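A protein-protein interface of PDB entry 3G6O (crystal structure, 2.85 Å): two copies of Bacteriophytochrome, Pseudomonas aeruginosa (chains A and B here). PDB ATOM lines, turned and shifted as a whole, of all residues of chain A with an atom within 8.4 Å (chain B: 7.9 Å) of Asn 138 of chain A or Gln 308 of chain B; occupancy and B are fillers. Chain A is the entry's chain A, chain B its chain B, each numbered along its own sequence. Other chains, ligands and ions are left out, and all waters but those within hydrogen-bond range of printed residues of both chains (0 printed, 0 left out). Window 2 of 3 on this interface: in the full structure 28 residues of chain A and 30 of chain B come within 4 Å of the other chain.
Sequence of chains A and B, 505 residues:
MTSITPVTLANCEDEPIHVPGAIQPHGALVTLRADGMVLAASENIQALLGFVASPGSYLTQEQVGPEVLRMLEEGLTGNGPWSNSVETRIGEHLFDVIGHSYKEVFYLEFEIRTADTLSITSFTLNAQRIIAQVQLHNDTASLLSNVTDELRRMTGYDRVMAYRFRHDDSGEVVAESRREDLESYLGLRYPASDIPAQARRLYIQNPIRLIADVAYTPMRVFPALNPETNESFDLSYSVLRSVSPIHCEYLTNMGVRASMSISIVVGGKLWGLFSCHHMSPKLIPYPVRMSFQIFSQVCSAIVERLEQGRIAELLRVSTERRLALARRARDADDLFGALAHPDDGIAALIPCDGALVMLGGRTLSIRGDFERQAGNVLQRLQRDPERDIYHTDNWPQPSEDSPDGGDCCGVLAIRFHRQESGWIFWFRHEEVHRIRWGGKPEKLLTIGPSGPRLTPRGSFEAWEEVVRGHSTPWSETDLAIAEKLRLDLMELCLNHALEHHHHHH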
ATOM      1  N   VAL A 134     -30.296   1.056  10.223  1.00  0.00           N
ATOM      2  CA  VAL A 134     -29.332   0.097   9.706  1.00  0.00           C
ATOM      3  C   VAL A 134     -29.248   0.069   8.180  1.00  0.00           C
ATOM      4  O   VAL A 134     -28.358  -0.558   7.617  1.00  0.00           O
ATOM      5  CB  VAL A 134     -29.617  -1.320  10.245  1.00  0.00           C
ATOM      6  CG1 VAL A 134     -29.656  -2.338   9.111  1.00  0.00           C
ATOM      7  CG2 VAL A 134     -28.592  -1.718  11.302  1.00  0.00           C
ATOM      8  N   GLN A 135     -30.152   0.759   7.504  1.00  0.00           N
ATOM      9  CA  GLN A 135     -30.207   0.638   6.053  1.00  0.00           C
ATOM     10  C   GLN A 135     -30.029   1.959   5.315  1.00  0.00           C
ATOM     11  O   GLN A 135     -30.332   2.060   4.117  1.00  0.00           O
ATOM     12  CB  GLN A 135     -31.515  -0.035   5.660  1.00  0.00           C
ATOM     13  CG  GLN A 135     -31.767  -1.309   6.466  1.00  0.00           C
ATOM     14  CD  GLN A 135     -33.194  -1.806   6.345  1.00  0.00           C
ATOM     15  OE1 GLN A 135     -34.132  -1.011   6.289  1.00  0.00           O
ATOM     16  NE2 GLN A 135     -33.368  -3.125   6.296  1.00  0.00           N
ATOM     17  N   LEU A 136     -29.515   2.963   6.024  1.00  0.00           N
ATOM     18  CA  LEU A 136     -29.219   4.258   5.420  1.00  0.00           C
ATOM     19  C   LEU A 136     -27.836   4.290   4.767  1.00  0.00           C
ATOM     20  O   LEU A 136     -27.558   5.152   3.928  1.00  0.00           O
ATOM     21  CB  LEU A 136     -29.312   5.373   6.467  1.00  0.00           C
ATOM     22  CG  LEU A 136     -30.707   5.727   6.974  1.00  0.00           C
ATOM     23  CD1 LEU A 136     -30.660   6.949   7.878  1.00  0.00           C
ATOM     24  CD2 LEU A 136     -31.650   5.962   5.802  1.00  0.00           C
ATOM     25  N   HIS A 137     -26.979   3.346   5.145  1.00  0.00           N
ATOM     26  CA  HIS A 137     -25.560   3.432   4.813  1.00  0.00           C
ATOM     27  C   HIS A 137     -25.015   2.191   4.103  1.00  0.00           C
ATOM     28  O   HIS A 137     -25.563   1.102   4.230  1.00  0.00           O
ATOM     29  CB  HIS A 137     -24.765   3.696   6.092  1.00  0.00           C
ATOM     30  CG  HIS A 137     -25.501   4.549   7.090  1.00  0.00           C
ATOM     31  ND1 HIS A 137     -26.333   4.010   8.042  1.00  0.00           N
ATOM     32  CD2 HIS A 137     -25.538   5.884   7.259  1.00  0.00           C
ATOM     33  CE1 HIS A 137     -26.853   4.989   8.775  1.00  0.00           C
ATOM     34  NE2 HIS A 137     -26.381   6.141   8.312  1.00  0.00           N
ATOM     35  N   ASN A 138     -23.930   2.373   3.350  1.00  0.00           N
ATOM     36  CA  ASN A 138     -23.231   1.270   2.685  1.00  0.00           C
ATOM     37  C   ASN A 138     -21.926   0.903   3.397  1.00  0.00           C
ATOM     38  O   ASN A 138     -21.557  -0.264   3.484  1.00  0.00           O
ATOM     39  CB  ASN A 138     -22.936   1.613   1.223  1.00  0.00           C
ATOM     40  CG  ASN A 138     -24.123   1.358   0.315  1.00  0.00           C
ATOM     41  OD1 ASN A 138     -25.175   1.984   0.456  1.00  0.00           O
ATOM     42  ND2 ASN A 138     -23.958   0.439  -0.632  1.00  0.00           N
ATOM     43  N   ASP A 139     -21.223   1.916   3.885  1.00  0.00           N
ATOM     44  CA  ASP A 139     -20.007   1.710   4.659  1.00  0.00           C
ATOM     45  C   ASP A 139     -20.359   0.940   5.927  1.00  0.00           C
ATOM     46  O   ASP A 139     -21.401   1.189   6.529  1.00  0.00           O
ATOM     47  CB  ASP A 139     -19.375   3.069   4.998  1.00  0.00           C
ATOM     48  CG  ASP A 139     -18.096   2.939   5.809  1.00  0.00           C
ATOM     49  OD1 ASP A 139     -17.606   1.802   5.988  1.00  0.00           O
ATOM     50  OD2 ASP A 139     -17.574   3.978   6.265  1.00  0.00           O
ATOM     51  N   THR A 140     -19.499   0.009   6.333  1.00  0.00           N
ATOM     52  CA  THR A 140     -19.733  -0.750   7.566  1.00  0.00           C
ATOM     53  C   THR A 140     -19.506   0.087   8.834  1.00  0.00           C
ATOM     54  O   THR A 140     -20.129  -0.158   9.860  1.00  0.00           O
ATOM     55  CB  THR A 140     -18.871  -2.033   7.650  1.00  0.00           C
ATOM     56  OG1 THR A 140     -19.555  -3.004   8.445  1.00  0.00           O
ATOM     57  CG2 THR A 140     -17.508  -1.741   8.286  1.00  0.00           C
ATOM     58  N   ALA A 141     -18.606   1.063   8.758  1.00  0.00           N
ATOM     59  CA  ALA A 141     -18.286   1.905   9.907  1.00  0.00           C
ATOM     60  C   ALA A 141     -19.410   2.879  10.221  1.00  0.00           C
ATOM     61  O   ALA A 141     -19.812   3.032  11.374  1.00  0.00           O
ATOM     62  CB  ALA A 141     -16.993   2.658   9.664  1.00  0.00           C
ATOM     63  N   SER A 142     -19.906   3.549   9.187  1.00  0.00           N
ATOM     64  CA  SER A 142     -21.009   4.486   9.343  1.00  0.00           C
ATOM     65  C   SER A 142     -22.201   3.749   9.928  1.00  0.00           C
ATOM     66  O   SER A 142     -22.881   4.262  10.817  1.00  0.00           O
ATOM     67  CB  SER A 142     -21.414   5.059   7.989  1.00  0.00           C
ATOM     68  OG  SER A 142     -20.323   5.037   7.088  1.00  0.00           O
ATOM     69  N   LEU A 143     -22.452   2.544   9.412  1.00  0.00           N
ATOM     70  CA  LEU A 143     -23.550   1.702   9.883  1.00  0.00           C
ATOM     71  C   LEU A 143     -23.480   1.503  11.390  1.00  0.00           C
ATOM     72  O   LEU A 143     -24.420   1.840  12.097  1.00  0.00           O
ATOM     73  CB  LEU A 143     -23.515   0.352   9.171  1.00  0.00           C
ATOM     74  CG  LEU A 143     -24.526  -0.761   9.485  1.00  0.00           C
ATOM     75  CD1 LEU A 143     -24.219  -1.496  10.796  1.00  0.00           C
ATOM     76  CD2 LEU A 143     -25.944  -0.228   9.472  1.00  0.00           C
ATOM     77  N   ILE A 302     -27.480  -7.778   7.066  1.00  0.00           N
ATOM     78  CA  ILE A 302     -27.022  -6.544   6.451  1.00  0.00           C
ATOM     79  C   ILE A 302     -25.484  -6.490   6.413  1.00  0.00           C
ATOM     80  O   ILE A 302     -24.900  -6.275   5.348  1.00  0.00           O
ATOM     81  CB  ILE A 302     -27.626  -5.298   7.176  1.00  0.00           C
ATOM     82  CG1 ILE A 302     -28.875  -4.775   6.460  1.00  0.00           C
ATOM     83  CG2 ILE A 302     -26.630  -4.178   7.258  1.00  0.00           C
ATOM     84  CD1 ILE A 302     -30.117  -5.618   6.660  1.00  0.00           C
ATOM     85  N   VAL A 303     -24.833  -6.725   7.555  1.00  0.00           N
ATOM     86  CA  VAL A 303     -23.370  -6.666   7.632  1.00  0.00           C
ATOM     87  C   VAL A 303     -22.692  -7.774   6.832  1.00  0.00           C
ATOM     88  O   VAL A 303     -21.627  -7.572   6.251  1.00  0.00           O
ATOM     89  CB  VAL A 303     -22.853  -6.739   9.085  1.00  0.00           C
ATOM     90  CG1 VAL A 303     -21.340  -6.776   9.087  1.00  0.00           C
ATOM     91  CG2 VAL A 303     -23.345  -5.552   9.879  1.00  0.00           C
ATOM     92  N   ARG A 305     -23.649  -9.190   3.980  1.00  0.00           N
ATOM     93  CA  ARG A 305     -23.578  -8.870   2.553  1.00  0.00           C
ATOM     94  C   ARG A 305     -22.642  -7.695   2.275  1.00  0.00           C
ATOM     95  O   ARG A 305     -21.866  -7.701   1.321  1.00  0.00           O
ATOM     96  CB  ARG A 305     -24.967  -8.637   1.957  1.00  0.00           C
ATOM     97  CG  ARG A 305     -25.620  -9.936   1.506  1.00  0.00           C
ATOM     98  CD  ARG A 305     -26.992  -9.716   0.905  1.00  0.00           C
ATOM     99  NE  ARG A 305     -27.894 -10.817   1.246  1.00  0.00           N
ATOM    100  CZ  ARG A 305     -29.143 -10.938   0.803  1.00  0.00           C
ATOM    101  NH1 ARG A 305     -29.649 -10.029  -0.012  1.00  0.00           N
ATOM    102  NH2 ARG A 305     -29.889 -11.972   1.175  1.00  0.00           N
ATOM    103  N   LEU A 306     -22.701  -6.708   3.150  1.00  0.00           N
ATOM    104  CA  LEU A 306     -21.839  -5.542   3.076  1.00  0.00           C
ATOM    105  C   LEU A 306     -20.363  -5.943   3.091  1.00  0.00           C
ATOM    106  O   LEU A 306     -19.545  -5.437   2.313  1.00  0.00           O
ATOM    107  CB  LEU A 306     -22.142  -4.658   4.278  1.00  0.00           C
ATOM    108  CG  LEU A 306     -22.420  -3.185   4.056  1.00  0.00           C
ATOM    109  CD1 LEU A 306     -23.149  -2.960   2.741  1.00  0.00           C
ATOM    110  CD2 LEU A 306     -23.232  -2.662   5.222  1.00  0.00           C
ATOM    111  N   GLU A 307     -20.035  -6.855   3.997  1.00  0.00           N
ATOM    112  CA  GLU A 307     -18.664  -7.299   4.213  1.00  0.00           C
ATOM    113  C   GLU A 307     -18.193  -8.309   3.174  1.00  0.00           C
ATOM    114  O   GLU A 307     -17.000  -8.439   2.950  1.00  0.00           O
ATOM    115  CB  GLU A 307     -18.526  -7.911   5.610  1.00  0.00           C
ATOM    116  CG  GLU A 307     -18.340  -6.898   6.706  1.00  0.00           C
ATOM    117  CD  GLU A 307     -17.043  -6.128   6.563  1.00  0.00           C
ATOM    118  OE1 GLU A 307     -15.984  -6.679   6.933  1.00  0.00           O
ATOM    119  OE2 GLU A 307     -17.085  -4.963   6.103  1.00  0.00           O
ATOM    120  N   ARG A 310     -17.561  -6.009   0.090  1.00  0.00           N
ATOM    121  CA  ARG A 310     -16.306  -5.321   0.347  1.00  0.00           C
ATOM    122  C   ARG A 310     -15.112  -6.217   0.047  1.00  0.00           C
ATOM    123  O   ARG A 310     -14.264  -5.887  -0.786  1.00  0.00           O
ATOM    124  CB  ARG A 310     -16.240  -4.853   1.801  1.00  0.00           C
ATOM    125  CG  ARG A 310     -14.974  -4.069   2.141  1.00  0.00           C
ATOM    126  CD  ARG A 310     -14.948  -3.629   3.599  1.00  0.00           C
ATOM    127  NE  ARG A 310     -14.603  -4.718   4.510  1.00  0.00           N
ATOM    128  CZ  ARG A 310     -13.353  -5.033   4.845  1.00  0.00           C
ATOM    129  NH1 ARG A 310     -12.335  -4.346   4.333  1.00  0.00           N
ATOM    130  NH2 ARG A 310     -13.113  -6.033   5.686  1.00  0.00           N
ATOM    131  N   VAL B 266     -37.914   0.693  -3.798  1.00  0.00           N
ATOM    132  CA  VAL B 266     -36.540   1.153  -4.008  1.00  0.00           C
ATOM    133  C   VAL B 266     -36.559   2.530  -4.687  1.00  0.00           C
ATOM    134  O   VAL B 266     -37.457   2.837  -5.483  1.00  0.00           O
ATOM    135  CB  VAL B 266     -35.720   0.158  -4.856  1.00  0.00           C
ATOM    136  CG1 VAL B 266     -35.983  -1.280  -4.407  1.00  0.00           C
ATOM    137  CG2 VAL B 266     -36.053   0.322  -6.324  1.00  0.00           C
ATOM    138  N   GLY B 267     -35.567   3.360  -4.379  1.00  0.00           N
ATOM    139  CA  GLY B 267     -35.666   4.773  -4.690  1.00  0.00           C
ATOM    140  C   GLY B 267     -36.865   5.228  -3.890  1.00  0.00           C
ATOM    141  O   GLY B 267     -37.069   4.756  -2.778  1.00  0.00           O
ATOM    142  N   ALA B 301     -35.214  -3.010   1.612  1.00  0.00           N
ATOM    143  CA  ALA B 301     -33.821  -2.605   1.736  1.00  0.00           C
ATOM    144  C   ALA B 301     -32.912  -3.666   1.143  1.00  0.00           C
ATOM    145  O   ALA B 301     -32.099  -3.378   0.263  1.00  0.00           O
ATOM    146  CB  ALA B 301     -33.472  -2.365   3.193  1.00  0.00           C
ATOM    147  N   ILE B 302     -33.049  -4.898   1.632  1.00  0.00           N
ATOM    148  CA  ILE B 302     -32.248  -6.009   1.140  1.00  0.00           C
ATOM    149  C   ILE B 302     -32.222  -6.016  -0.396  1.00  0.00           C
ATOM    150  O   ILE B 302     -31.168  -6.217  -1.005  1.00  0.00           O
ATOM    151  CB  ILE B 302     -32.781  -7.355   1.671  1.00  0.00           C
ATOM    152  CG1 ILE B 302     -32.264  -7.628   3.083  1.00  0.00           C
ATOM    153  CG2 ILE B 302     -32.352  -8.483   0.778  1.00  0.00           C
ATOM    154  CD1 ILE B 302     -32.449  -6.478   4.041  1.00  0.00           C
ATOM    155  N   VAL B 303     -33.378  -5.776  -1.017  1.00  0.00           N
ATOM    156  CA  VAL B 303     -33.477  -5.700  -2.478  1.00  0.00           C
ATOM    157  C   VAL B 303     -32.754  -4.493  -3.084  1.00  0.00           C
ATOM    158  O   VAL B 303     -32.142  -4.601  -4.147  1.00  0.00           O
ATOM    159  CB  VAL B 303     -34.938  -5.671  -2.963  1.00  0.00           C
ATOM    160  CG1 VAL B 303     -34.997  -5.205  -4.409  1.00  0.00           C
ATOM    161  CG2 VAL B 303     -35.572  -7.038  -2.814  1.00  0.00           C
ATOM    162  N   GLU B 304     -32.839  -3.346  -2.421  1.00  0.00           N
ATOM    163  CA  GLU B 304     -32.255  -2.123  -2.949  1.00  0.00           C
ATOM    164  C   GLU B 304     -30.750  -2.241  -3.027  1.00  0.00           C
ATOM    165  O   GLU B 304     -30.133  -1.780  -3.985  1.00  0.00           O
ATOM    166  CB  GLU B 304     -32.631  -0.918  -2.091  1.00  0.00           C
ATOM    167  CG  GLU B 304     -31.792   0.308  -2.379  1.00  0.00           C
ATOM    168  CD  GLU B 304     -32.525   1.591  -2.085  1.00  0.00           C
ATOM    169  OE1 GLU B 304     -33.758   1.533  -1.883  1.00  0.00           O
ATOM    170  OE2 GLU B 304     -31.868   2.653  -2.067  1.00  0.00           O
ATOM    171  N   ARG B 305     -30.151  -2.868  -2.025  1.00  0.00           N
ATOM    172  CA  ARG B 305     -28.704  -2.929  -2.006  1.00  0.00           C
ATOM    173  C   ARG B 305     -28.196  -3.986  -2.993  1.00  0.00           C
ATOM    174  O   ARG B 305     -27.182  -3.784  -3.662  1.00  0.00           O
ATOM    175  CB  ARG B 305     -28.182  -3.119  -0.578  1.00  0.00           C
ATOM    176  CG  ARG B 305     -26.916  -2.315  -0.308  1.00  0.00           C
ATOM    177  CD  ARG B 305     -26.355  -2.573   1.061  1.00  0.00           C
ATOM    178  NE  ARG B 305     -26.896  -1.661   2.060  1.00  0.00           N
ATOM    179  CZ  ARG B 305     -26.736  -1.831   3.368  1.00  0.00           C
ATOM    180  NH1 ARG B 305     -26.062  -2.884   3.818  1.00  0.00           N
ATOM    181  NH2 ARG B 305     -27.252  -0.961   4.224  1.00  0.00           N
ATOM    182  N   LEU B 306     -28.929  -5.090  -3.106  1.00  0.00           N
ATOM    183  CA  LEU B 306     -28.626  -6.124  -4.102  1.00  0.00           C
ATOM    184  C   LEU B 306     -28.628  -5.577  -5.523  1.00  0.00           C
ATOM    185  O   LEU B 306     -27.799  -5.963  -6.349  1.00  0.00           O
ATOM    186  CB  LEU B 306     -29.663  -7.238  -4.050  1.00  0.00           C
ATOM    187  CG  LEU B 306     -29.252  -8.495  -3.320  1.00  0.00           C
ATOM    188  CD1 LEU B 306     -28.542  -8.115  -2.033  1.00  0.00           C
ATOM    189  CD2 LEU B 306     -30.474  -9.328  -3.041  1.00  0.00           C
ATOM    190  N   GLU B 307     -29.581  -4.700  -5.813  1.00  0.00           N
ATOM    191  CA  GLU B 307     -29.780  -4.229  -7.170  1.00  0.00           C
ATOM    192  C   GLU B 307     -28.812  -3.106  -7.523  1.00  0.00           C
ATOM    193  O   GLU B 307     -28.418  -2.948  -8.678  1.00  0.00           O
ATOM    194  CB  GLU B 307     -31.232  -3.793  -7.361  1.00  0.00           C
ATOM    195  CG  GLU B 307     -32.191  -4.953  -7.541  1.00  0.00           C
ATOM    196  CD  GLU B 307     -32.215  -5.477  -8.962  1.00  0.00           C
ATOM    197  OE1 GLU B 307     -32.668  -4.734  -9.862  1.00  0.00           O
ATOM    198  OE2 GLU B 307     -31.802  -6.639  -9.174  1.00  0.00           O
ATOM    199  N   GLN B 308     -28.416  -2.328  -6.527  1.00  0.00           N
ATOM    200  CA  GLN B 308     -27.456  -1.276  -6.810  1.00  0.00           C
ATOM    201  C   GLN B 308     -26.082  -1.911  -7.004  1.00  0.00           C
ATOM    202  O   GLN B 308     -25.270  -1.426  -7.791  1.00  0.00           O
ATOM    203  CB  GLN B 308     -27.464  -0.182  -5.735  1.00  0.00           C
ATOM    204  CG  GLN B 308     -26.799  -0.542  -4.420  1.00  0.00           C
ATOM    205  CD  GLN B 308     -27.179   0.430  -3.313  1.00  0.00           C
ATOM    206  OE1 GLN B 308     -26.681   0.345  -2.189  1.00  0.00           O
ATOM    207  NE2 GLN B 308     -28.076   1.358  -3.631  1.00  0.00           N
ATOM    208  N   GLY B 309     -25.851  -3.023  -6.314  1.00  0.00           N
ATOM    209  CA  GLY B 309     -24.626  -3.786  -6.494  1.00  0.00           C
ATOM    210  C   GLY B 309     -24.576  -4.404  -7.880  1.00  0.00           C
ATOM    211  O   GLY B 309     -23.609  -4.227  -8.617  1.00  0.00           O
ATOM    212  N   ARG B 310     -25.632  -5.131  -8.226  1.00  0.00           N
ATOM    213  CA  ARG B 310     -25.761  -5.743  -9.536  1.00  0.00           C
ATOM    214  C   ARG B 310     -25.513  -4.707 -10.629  1.00  0.00           C
ATOM    215  O   ARG B 310     -24.677  -4.906 -11.514  1.00  0.00           O
ATOM    216  CB  ARG B 310     -27.162  -6.345  -9.699  1.00  0.00           C
ATOM    217  CG  ARG B 310     -27.380  -7.088 -11.025  1.00  0.00           C
ATOM    218  CD  ARG B 310     -28.786  -7.670 -11.162  1.00  0.00           C
ATOM    219  NE  ARG B 310     -29.823  -6.650 -11.290  1.00  0.00           N
ATOM    220  CZ  ARG B 310     -30.256  -6.174 -12.454  1.00  0.00           C
ATOM    221  NH1 ARG B 310     -29.727  -6.622 -13.594  1.00  0.00           N
ATOM    222  NH2 ARG B 310     -31.213  -5.253 -12.484  1.00  0.00           N
ATOM    223  N   ILE B 311     -26.255  -3.607 -10.564  1.00  0.00           N
ATOM    224  CA  ILE B 311     -26.189  -2.582 -11.598  1.00  0.00           C
ATOM    225  C   ILE B 311     -24.847  -1.881 -11.576  1.00  0.00           C
ATOM    226  O   ILE B 311     -24.321  -1.491 -12.618  1.00  0.00           O
ATOM    227  CB  ILE B 311     -27.298  -1.535 -11.438  1.00  0.00           C
ATOM    228  CG1 ILE B 311     -28.675  -2.206 -11.529  1.00  0.00           C
ATOM    229  CG2 ILE B 311     -27.155  -0.480 -12.500  1.00  0.00           C
ATOM    230  CD1 ILE B 311     -29.838  -1.286 -11.162  1.00  0.00           C
ATOM    231  N   ALA B 312     -24.290  -1.729 -10.382  1.00  0.00           N
ATOM    232  CA  ALA B 312     -22.988  -1.094 -10.252  1.00  0.00           C
ATOM    233  C   ALA B 312     -21.935  -1.938 -10.960  1.00  0.00           C
ATOM    234  O   ALA B 312     -20.865  -1.447 -11.321  1.00  0.00           O
ATOM    235  CB  ALA B 312     -22.625  -0.928  -8.794  1.00  0.00           C
ATOM    236  N   GLU B 313     -22.254  -3.215 -11.144  1.00  0.00           N
ATOM    237  CA  GLU B 313     -21.323  -4.175 -11.721  1.00  0.00           C
ATOM    238  C   GLU B 313     -21.405  -4.203 -13.236  1.00  0.00           C
ATOM    239  O   GLU B 313     -20.390  -4.104 -13.920  1.00  0.00           O
ATOM    240  CB  GLU B 313     -21.578  -5.573 -11.153  1.00  0.00           C
ATOM    241  CG  GLU B 313     -20.772  -6.669 -11.818  1.00  0.00           C
ATOM    242  CD  GLU B 313     -19.296  -6.617 -11.456  1.00  0.00           C
ATOM    243  OE1 GLU B 313     -18.897  -5.807 -10.587  1.00  0.00           O
ATOM    244  OE2 GLU B 313     -18.521  -7.398 -12.043  1.00  0.00           O
ATOM    245  N   LEU B 314     -22.612  -4.356 -13.759  1.00  0.00           N
ATOM    246  CA  LEU B 314     -22.815  -4.280 -15.202  1.00  0.00           C
ATOM    247  C   LEU B 314     -22.187  -2.995 -15.694  1.00  0.00           C
ATOM    248  O   LEU B 314     -21.473  -2.976 -16.703  1.00  0.00           O
ATOM    249  CB  LEU B 314     -24.305  -4.277 -15.553  1.00  0.00           C
ATOM    250  CG  LEU B 314     -25.142  -5.395 -14.945  1.00  0.00           C
ATOM    251  CD1 LEU B 314     -26.499  -5.501 -15.618  1.00  0.00           C
ATOM    252  CD2 LEU B 314     -24.392  -6.693 -15.078  1.00  0.00           C
ATOM    253  N   LEU B 315     -22.451  -1.920 -14.958  1.00  0.00           N
ATOM    254  CA  LEU B 315     -21.989  -0.589 -15.329  1.00  0.00           C
ATOM    255  C   LEU B 315     -20.473  -0.511 -15.376  1.00  0.00           C
ATOM    256  O   LEU B 315     -19.907   0.298 -16.109  1.00  0.00           O
ATOM    257  CB  LEU B 315     -22.520   0.446 -14.352  1.00  0.00           C
ATOM    258  CG  LEU B 315     -22.446   1.851 -14.921  1.00  0.00           C
ATOM    259  CD1 LEU B 315     -23.092   1.864 -16.290  1.00  0.00           C
ATOM    260  CD2 LEU B 315     -23.105   2.855 -13.995  1.00  0.00           C
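Of the 16 printed residues of chain A, 7 touch a printed residue of chain B.
Hydrophobic or aromatic side chains of chain A within 4 Å of the printed part of chain B: Ile 302 and Leu 306.
Hydrophobic or aromatic side chains of chain B that line the printed part of chain A: Ala 301, Ile 302 and Leu 306.
Among the printed residues, 10 pairs touch across the chains.
Among the printed residues, no Asp or Glu carboxylate lies within 4 Å of a Lys or Arg side-chain nitrogen of the other chain.
NH2 of Arg 305 of chain B is in hydrogen-bond range of O of His 137 of chain A (2.7 Å).
The side-chain amide nitrogen of Asn 138 of chain A lies within hydrogen-bond range of the side-chain amide oxygen of Gln 308 of chain B (3.1 Å).
Ile 302 of chain A touches its own counterpart, Ile 302 of chain B.
Ile 302 of chain A touches Arg 305 of chain B, and with the chains exchanged Arg 305 of chain A touches Ile 302 of chain B.
Arg 305 of chain A touches Leu 306 of chain B, and with the chains exchanged Leu 306 of chain A touches Arg 305 of chain B.
6 positions are printed for both chains.
Of the 10 pairs that touch across the chains among the printed residues, 5 have their exchanged pair printed and touching as well.
Val 134 of chain A touches Arg 305 of chain B (O to NH2, 3.6 Å).
Gln 135 of chain A touches Ala 301 of chain B.
NH2 of Arg 305 of chain B touches CA of Gln 135 of chain A, 3.8 Å away.
Ile 302 of chain A touches Ile 302 of chain B.
NH1 of Arg 305 of chain B touches CG2 of Ile 302 of chain A (3.7 Å).
Arg 305 of chain A touches Ile 302 of chain B.
CD1 of Leu 306 of chain B touches NH1 of Arg 305 of chain A (3.0 Å).
Leu 306 of chain A touches Arg 305 of chain B.
Of the printed residues of chain B, Val 134 of chain A touches Arg 305.
Of the printed residues of chain B, Gln 135 of chain A touches Ala 301 and Arg 305.
Of the printed residues of chain B, His 137 of chain A touches Arg 305 (2.7 Å).
Gln 308 of chain B touches one residue of chain A.
No residue of chain A comes within 4 Å of Gly 309 of chain B.
The nearest residue of chain A that does not touch Gln 308 of chain B is His 137 of chain A (6.6 Å).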
